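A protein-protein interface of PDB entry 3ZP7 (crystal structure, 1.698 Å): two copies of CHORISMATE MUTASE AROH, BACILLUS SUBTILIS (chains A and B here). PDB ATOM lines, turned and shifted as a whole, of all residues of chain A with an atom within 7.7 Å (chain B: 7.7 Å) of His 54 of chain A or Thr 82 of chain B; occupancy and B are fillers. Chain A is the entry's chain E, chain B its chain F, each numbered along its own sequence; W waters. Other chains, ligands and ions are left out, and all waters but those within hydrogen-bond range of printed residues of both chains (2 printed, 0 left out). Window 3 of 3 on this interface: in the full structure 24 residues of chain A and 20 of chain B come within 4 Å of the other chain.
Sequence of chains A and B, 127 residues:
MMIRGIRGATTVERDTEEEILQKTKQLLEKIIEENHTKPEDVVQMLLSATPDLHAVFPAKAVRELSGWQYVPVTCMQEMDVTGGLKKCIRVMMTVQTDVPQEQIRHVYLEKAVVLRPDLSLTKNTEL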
ATOM      1  N   ASP A  15      -8.437 -18.356 -21.713  1.00  0.00           N
ATOM      2  CA  ASP A  15      -8.724 -19.765 -21.905  1.00  0.00           C
ATOM      3  C   ASP A  15      -8.641 -20.140 -23.390  1.00  0.00           C
ATOM      4  O   ASP A  15      -9.656 -20.290 -24.056  1.00  0.00           O
ATOM      5  CB  ASP A  15     -10.104 -20.104 -21.313  1.00  0.00           C
ATOM      6  CG  ASP A  15     -10.468 -21.576 -21.476  1.00  0.00           C
ATOM      7  OD1 ASP A  15      -9.546 -22.407 -21.608  1.00  0.00           O
ATOM      8  OD2 ASP A  15     -11.675 -21.895 -21.472  1.00  0.00           O
ATOM      9  N   THR A  16      -7.425 -20.248 -23.918  1.00  0.00           N
ATOM     10  CA  THR A  16      -7.245 -20.660 -25.307  1.00  0.00           C
ATOM     11  C   THR A  16      -6.274 -21.820 -25.410  1.00  0.00           C
ATOM     12  O   THR A  16      -5.439 -22.021 -24.528  1.00  0.00           O
ATOM     13  CB  THR A  16      -6.700 -19.523 -26.199  1.00  0.00           C
ATOM     14  OG1 THR A  16      -5.384 -19.147 -25.757  1.00  0.00           O
ATOM     15  CG2 THR A  16      -7.633 -18.320 -26.171  1.00  0.00           C
ATOM     16  N   GLU A  17      -6.369 -22.570 -26.501  1.00  0.00           N
ATOM     17  CA  GLU A  17      -5.488 -23.710 -26.687  1.00  0.00           C
ATOM     18  C   GLU A  17      -4.031 -23.267 -26.751  1.00  0.00           C
ATOM     19  O   GLU A  17      -3.162 -23.851 -26.098  1.00  0.00           O
ATOM     20  CB  GLU A  17      -5.870 -24.468 -27.951  1.00  0.00           C
ATOM     21  CG  GLU A  17      -5.007 -25.663 -28.222  1.00  0.00           C
ATOM     22  CD  GLU A  17      -5.653 -26.610 -29.189  1.00  0.00           C
ATOM     23  OE1 GLU A  17      -6.878 -26.472 -29.413  1.00  0.00           O
ATOM     24  OE2 GLU A  17      -4.939 -27.487 -29.719  1.00  0.00           O
ATOM     25  N   ILE A  20      -2.761 -22.210 -23.157  1.00  0.00           N
ATOM     26  CA  ILE A  20      -2.665 -23.371 -22.268  1.00  0.00           C
ATOM     27  C   ILE A  20      -1.482 -24.279 -22.650  1.00  0.00           C
ATOM     28  O   ILE A  20      -0.668 -24.662 -21.797  1.00  0.00           O
ATOM     29  CB  ILE A  20      -3.993 -24.179 -22.235  1.00  0.00           C
ATOM     30  CG1 ILE A  20      -5.097 -23.351 -21.568  1.00  0.00           C
ATOM     31  CG2 ILE A  20      -3.799 -25.486 -21.466  1.00  0.00           C
ATOM     32  CD1 ILE A  20      -6.492 -23.968 -21.656  1.00  0.00           C
ATOM     33  N   ALA A  49      -6.268 -28.097 -13.647  1.00  0.00           N
ATOM     34  CA  ALA A  49      -6.624 -26.750 -14.068  1.00  0.00           C
ATOM     35  C   ALA A  49      -7.788 -26.261 -13.230  1.00  0.00           C
ATOM     36  O   ALA A  49      -8.689 -27.022 -12.898  1.00  0.00           O
ATOM     37  CB  ALA A  49      -7.009 -26.724 -15.538  1.00  0.00           C
ATOM     38  N   THR A  50      -7.774 -24.981 -12.895  1.00  0.00           N
ATOM     39  CA  THR A  50      -8.928 -24.380 -12.237  1.00  0.00           C
ATOM     40  C   THR A  50     -10.139 -24.433 -13.175  1.00  0.00           C
ATOM     41  O   THR A  50      -9.983 -24.579 -14.386  1.00  0.00           O
ATOM     42  CB  THR A  50      -8.625 -22.928 -11.816  1.00  0.00           C
ATOM     43  OG1 THR A  50      -7.965 -22.252 -12.886  1.00  0.00           O
ATOM     44  CG2 THR A  50      -7.722 -22.915 -10.591  1.00  0.00           C
ATOM     45  N   PRO A  51     -11.355 -24.347 -12.614  1.00  0.00           N
ATOM     46  CA  PRO A  51     -12.541 -24.621 -13.439  1.00  0.00           C
ATOM     47  C   PRO A  51     -12.930 -23.488 -14.380  1.00  0.00           C
ATOM     48  O   PRO A  51     -14.019 -23.540 -14.958  1.00  0.00           O
ATOM     49  CB  PRO A  51     -13.642 -24.862 -12.403  1.00  0.00           C
ATOM     50  CG  PRO A  51     -13.178 -24.165 -11.175  1.00  0.00           C
ATOM     51  CD  PRO A  51     -11.683 -24.305 -11.177  1.00  0.00           C
ATOM     52  N   ASP A  52     -12.074 -22.478 -14.511  1.00  0.00           N
ATOM     53  CA  ASP A  52     -12.260 -21.433 -15.524  1.00  0.00           C
ATOM     54  C   ASP A  52     -11.496 -21.733 -16.824  1.00  0.00           C
ATOM     55  O   ASP A  52     -11.525 -20.932 -17.771  1.00  0.00           O
ATOM     56  CB  ASP A  52     -11.849 -20.059 -14.976  1.00  0.00           C
ATOM     57  CG  ASP A  52     -10.511 -20.090 -14.259  1.00  0.00           C
ATOM     58  OD1 ASP A  52      -9.777 -21.095 -14.386  1.00  0.00           O
ATOM     59  OD2 ASP A  52     -10.201 -19.102 -13.557  1.00  0.00           O
ATOM     60  N   LEU A  53     -10.831 -22.885 -16.878  1.00  0.00           N
ATOM     61  CA  LEU A  53     -10.113 -23.307 -18.084  1.00  0.00           C
ATOM     62  C   LEU A  53     -10.737 -24.557 -18.706  1.00  0.00           C
ATOM     63  O   LEU A  53     -10.849 -25.602 -18.048  1.00  0.00           O
ATOM     64  CB  LEU A  53      -8.621 -23.526 -17.783  1.00  0.00           C
ATOM     65  CG  LEU A  53      -7.906 -22.301 -17.209  1.00  0.00           C
ATOM     66  CD1 LEU A  53      -6.483 -22.665 -16.827  1.00  0.00           C
ATOM     67  CD2 LEU A  53      -7.905 -21.128 -18.193  1.00  0.00           C
ATOM     68  N   HIS A  54     -11.163 -24.443 -19.967  1.00  0.00           N
ATOM     69  CA  HIS A  54     -11.837 -25.546 -20.663  1.00  0.00           C
ATOM     70  C   HIS A  54     -11.348 -25.800 -22.090  1.00  0.00           C
ATOM     71  O   HIS A  54     -11.818 -26.739 -22.731  1.00  0.00           O
ATOM     72  CB  HIS A  54     -13.339 -25.273 -20.724  1.00  0.00           C
ATOM     73  CG  HIS A  54     -13.932 -24.921 -19.397  1.00  0.00           C
ATOM     74  ND1 HIS A  54     -14.195 -25.866 -18.431  1.00  0.00           N
ATOM     75  CD2 HIS A  54     -14.284 -23.727 -18.863  1.00  0.00           C
ATOM     76  CE1 HIS A  54     -14.700 -25.274 -17.363  1.00  0.00           C
ATOM     77  NE2 HIS A  54     -14.768 -23.975 -17.600  1.00  0.00           N
ATOM     78  N   ALA A  55     -10.438 -24.967 -22.600  1.00  0.00           N
ATOM     79  CA  ALA A  55     -10.122 -25.016 -24.039  1.00  0.00           C
ATOM     80  C   ALA A  55      -9.481 -26.318 -24.521  1.00  0.00           C
ATOM     81  O   ALA A  55      -9.781 -26.798 -25.626  1.00  0.00           O
ATOM     82  CB  ALA A  55      -9.234 -23.823 -24.453  1.00  0.00           C
ATOM     83  N   VAL A  56      -8.589 -26.877 -23.711  1.00  0.00           N
ATOM     84  CA  VAL A  56      -7.809 -28.048 -24.109  1.00  0.00           C
ATOM     85  C   VAL A  56      -7.251 -28.706 -22.838  1.00  0.00           C
ATOM     86  O   VAL A  56      -7.096 -28.036 -21.830  1.00  0.00           O
ATOM     87  CB  VAL A  56      -6.628 -27.638 -25.036  1.00  0.00           C
ATOM     88  CG1 VAL A  56      -5.595 -26.792 -24.274  1.00  0.00           C
ATOM     89  CG2 VAL A  56      -5.967 -28.854 -25.677  1.00  0.00           C
ATOM     90  N   PHE A  57      -6.963 -30.007 -22.870  1.00  0.00           N
ATOM     91  CA  PHE A  57      -6.256 -30.643 -21.750  1.00  0.00           C
ATOM     92  C   PHE A  57      -4.790 -30.205 -21.756  1.00  0.00           C
ATOM     93  O   PHE A  57      -4.134 -30.317 -22.784  1.00  0.00           O
ATOM     94  CB  PHE A  57      -6.292 -32.170 -21.882  1.00  0.00           C
ATOM     95  CG  PHE A  57      -7.629 -32.786 -21.590  1.00  0.00           C
ATOM     96  CD1 PHE A  57      -8.076 -32.913 -20.285  1.00  0.00           C
ATOM     97  CD2 PHE A  57      -8.431 -33.261 -22.623  1.00  0.00           C
ATOM     98  CE1 PHE A  57      -9.296 -33.491 -20.006  1.00  0.00           C
ATOM     99  CE2 PHE A  57      -9.662 -33.837 -22.353  1.00  0.00           C
ATOM    100  CZ  PHE A  57     -10.096 -33.954 -21.040  1.00  0.00           C
ATOM    101  N   GLN A  77      -9.614 -31.716 -12.272  1.00  0.00           N
ATOM    102  CA  GLN A  77     -10.082 -30.366 -11.965  1.00  0.00           C
ATOM    103  C   GLN A  77      -9.626 -29.919 -10.582  1.00  0.00           C
ATOM    104  O   GLN A  77      -9.728 -30.654  -9.600  1.00  0.00           O
ATOM    105  CB  GLN A  77     -11.602 -30.260 -12.091  1.00  0.00           C
ATOM    106  CG  GLN A  77     -12.130 -28.833 -11.903  1.00  0.00           C
ATOM    107  CD  GLN A  77     -13.616 -28.706 -12.169  1.00  0.00           C
ATOM    108  OE1 GLN A  77     -14.071 -28.820 -13.309  1.00  0.00           O
ATOM    109  NE2 GLN A  77     -14.382 -28.457 -11.120  1.00  0.00           N
ATOM    110  N   GLN B  77     -12.660 -35.538 -10.069  1.00  0.00           N
ATOM    111  CA  GLN B  77     -13.361 -35.110 -11.270  1.00  0.00           C
ATOM    112  C   GLN B  77     -12.350 -34.803 -12.362  1.00  0.00           C
ATOM    113  O   GLN B  77     -11.383 -34.093 -12.132  1.00  0.00           O
ATOM    114  CB  GLN B  77     -14.220 -33.873 -11.010  1.00  0.00           C
ATOM    115  CG  GLN B  77     -15.107 -33.538 -12.222  1.00  0.00           C
ATOM    116  CD  GLN B  77     -15.727 -32.154 -12.171  1.00  0.00           C
ATOM    117  OE1 GLN B  77     -16.647 -31.903 -11.389  1.00  0.00           O
ATOM    118  NE2 GLN B  77     -15.242 -31.253 -13.032  1.00  0.00           N
ATOM    119  N   MET B  79     -10.996 -32.853 -15.557  1.00  0.00           N
ATOM    120  CA  MET B  79     -11.137 -31.526 -16.111  1.00  0.00           C
ATOM    121  C   MET B  79     -12.238 -31.504 -17.185  1.00  0.00           C
ATOM    122  O   MET B  79     -12.344 -32.422 -18.001  1.00  0.00           O
ATOM    123  CB  MET B  79      -9.788 -31.127 -16.699  1.00  0.00           C
ATOM    124  CG  MET B  79      -9.712 -29.729 -17.177  1.00  0.00           C
ATOM    125  SD  MET B  79      -8.107 -29.464 -17.909  1.00  0.00           S
ATOM    126  CE  MET B  79      -8.421 -27.888 -18.697  1.00  0.00           C
ATOM    127  N   ASP B  80     -13.073 -30.469 -17.154  1.00  0.00           N
ATOM    128  CA  ASP B  80     -14.142 -30.289 -18.131  1.00  0.00           C
ATOM    129  C   ASP B  80     -13.622 -29.547 -19.362  1.00  0.00           C
ATOM    130  O   ASP B  80     -13.448 -28.330 -19.338  1.00  0.00           O
ATOM    131  CB  ASP B  80     -15.314 -29.532 -17.504  1.00  0.00           C
ATOM    132  CG  ASP B  80     -16.569 -29.559 -18.369  1.00  0.00           C
ATOM    133  OD1 ASP B  80     -16.655 -30.400 -19.290  1.00  0.00           O
ATOM    134  OD2 ASP B  80     -17.481 -28.744 -18.113  1.00  0.00           O
ATOM    135  N   VAL B  81     -13.381 -30.294 -20.432  1.00  0.00           N
ATOM    136  CA  VAL B  81     -12.827 -29.728 -21.657  1.00  0.00           C
ATOM    137  C   VAL B  81     -13.871 -29.616 -22.758  1.00  0.00           C
ATOM    138  O   VAL B  81     -14.626 -30.557 -23.015  1.00  0.00           O
ATOM    139  CB  VAL B  81     -11.607 -30.533 -22.129  1.00  0.00           C
ATOM    140  CG1 VAL B  81     -11.140 -30.070 -23.513  1.00  0.00           C
ATOM    141  CG2 VAL B  81     -10.488 -30.369 -21.115  1.00  0.00           C
ATOM    142  N   THR B  82     -13.906 -28.442 -23.382  1.00  0.00           N
ATOM    143  CA  THR B  82     -14.844 -28.132 -24.445  1.00  0.00           C
ATOM    144  C   THR B  82     -14.625 -29.086 -25.615  1.00  0.00           C
ATOM    145  O   THR B  82     -13.555 -29.102 -26.226  1.00  0.00           O
ATOM    146  CB  THR B  82     -14.665 -26.679 -24.927  1.00  0.00           C
ATOM    147  OG1 THR B  82     -14.860 -25.773 -23.830  1.00  0.00           O
ATOM    148  CG2 THR B  82     -15.653 -26.352 -26.016  1.00  0.00           C
ATOM    149  N   GLY B  83     -15.637 -29.896 -25.909  1.00  0.00           N
ATOM    150  CA  GLY B  83     -15.549 -30.857 -26.993  1.00  0.00           C
ATOM    151  C   GLY B  83     -14.880 -32.163 -26.593  1.00  0.00           C
ATOM    152  O   GLY B  83     -14.704 -33.056 -27.420  1.00  0.00           O
ATOM    153  N   GLY B  84     -14.501 -32.277 -25.326  1.00  0.00           N
ATOM    154  CA  GLY B  84     -13.857 -33.487 -24.836  1.00  0.00           C
ATOM    155  C   GLY B  84     -14.746 -34.718 -24.916  1.00  0.00           C
ATOM    156  O   GLY B  84     -15.963 -34.618 -25.073  1.00  0.00           O
ATOM    157  N   LEU B  85     -14.137 -35.891 -24.816  1.00  0.00           N
ATOM    158  CA  LEU B  85     -14.905 -37.128 -24.792  1.00  0.00           C
ATOM    159  C   LEU B  85     -15.852 -37.129 -23.592  1.00  0.00           C
ATOM    160  O   LEU B  85     -15.440 -36.837 -22.467  1.00  0.00           O
ATOM    161  CB  LEU B  85     -13.957 -38.316 -24.719  1.00  0.00           C
ATOM    162  CG  LEU B  85     -14.573 -39.712 -24.770  1.00  0.00           C
ATOM    163  CD1 LEU B  85     -15.401 -39.881 -26.033  1.00  0.00           C
ATOM    164  CD2 LEU B  85     -13.465 -40.739 -24.719  1.00  0.00           C
ATOM    165  N   LYS B  86     -17.126 -37.419 -23.836  1.00  0.00           N
ATOM    166  CA  LYS B  86     -18.110 -37.452 -22.752  1.00  0.00           C
ATOM    167  C   LYS B  86     -18.218 -38.820 -22.076  1.00  0.00           C
ATOM    168  O   LYS B  86     -17.766 -39.834 -22.616  1.00  0.00           O
ATOM    169  CB  LYS B  86     -19.489 -37.029 -23.256  1.00  0.00           C
ATOM    170  CG  LYS B  86     -19.536 -35.654 -23.895  1.00  0.00           C
ATOM    171  CD  LYS B  86     -19.109 -34.563 -22.924  1.00  0.00           C
ATOM    172  CE  LYS B  86     -19.003 -33.213 -23.628  1.00  0.00           C
ATOM    173  NZ  LYS B  86     -17.917 -32.380 -23.040  1.00  0.00           N
HETATM  174  O   HOH W   1     -13.092 -23.306 -23.798  1.00  0.00           O
HETATM  175  O   HOH W   2     -13.186 -27.717 -15.940  1.00  0.00           O
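The backbone carbonyl oxygen (O) of Asp 80 of chain B is in hydrogen-bond range of a ring nitrogen (ND1) of His 54 of chain A (2.7 Å). The backbone carbonyl oxygen of His 54 of chain A sits at hydrogen-bond distance from the backbone NH of Thr 82 of chain B, 2.8 Å away. NE2 of Gln 77 of chain B lies within hydrogen-bond range of OE1 of Gln 77 of chain A (2.7 Å).
Gln 77 of chain B touches its own counterpart, Gln 77 of chain A. Position printed for both chains: 77. Of the 12 pairs that touch across the chains among the printed residues, 1 has its exchanged pair printed and touching as well.
Met 79 of chain B touches Ala 49 of chain A (CE to CB, 3.7 Å). Leu 53 of chain A touches Met 79 of chain B. Leu 53 of chain A touches Asp 80 of chain B (O to O, 3.98 Å). Val 81 of chain B touches His 54 of chain A. Met 79 of chain B touches Val 56 of chain A. Val 56 of chain A touches Val 81 of chain B. Phe 57 of chain A touches Met 79 of chain B. Val 81 of chain B touches Phe 57 of chain A. Gln 77 of chain A touches Met 79 of chain B (N to N, 3.7 Å).
Printed residues of chain B within 4 Å of His 54 of chain A: Asp 80, Val 81 and Thr 82. Printed residues of chain B within 4 Å of Ala 49 of chain A: Met 79 (3.7 Å). Of the printed residues of chain B, Gln 77 of chain A touches Gln 77 (2.7 Å) and Met 79 (3.7 Å). Of the printed residues of chain A, Asp 80 of chain B touches Leu 53 (3.98 Å) and His 54 (2.7 Å). Of the printed residues of chain B, Leu 53 of chain A touches Met 79 and Asp 80. Leu 85 of chain B touches none of the printed residues of chain A. The nearest residue of chain A that does not touch Thr 82 of chain B is Ala 55 of chain A (4.5 Å).
The backbone NH of His 54 of chain A sits at hydrogen-bond distance from the side-chain carboxylate of Asp 15 of chain A (3.0 Å). NE2 of His 54 of chain A is in hydrogen-bond range of O of Pro 51 of chain A.
Of the 9 printed residues of chain B, 5 touch a printed residue of chain A. Hydrophobic or aromatic side chains of chain B within 4 Å of the printed part of chain A: Met 79 and Val 81. Along chain B the printed residues that touch a printed residue of chain A span positions 77 to 82. Hydrophobic or aromatic side chains of chain A that line the printed part of chain B: Ala 49, His 54 and Phe 57. Among the printed residues, 12 pairs touch across the chains. Among the printed residues, no Asp or Glu carboxylate lies within 4 Å of a Lys or Arg side-chain nitrogen of the other chain.
Water W2 lies within hydrogen-bond range of the side-chain amide oxygen of Gln 77 of chain A, the backbone NH of Asp 80 of chain B and a ring nitrogen (ND1) of His 54 of chain A. Water W1 lies within hydrogen-bond range of the side-chain hydroxyl (OG1) of Thr 82 of chain B (3.0 Å), the side-chain carboxylate (OD2) of Asp 15 of chain A (3.1 Å) and the backbone NH (N) of Ala 55 of chain A (3.4 Å).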
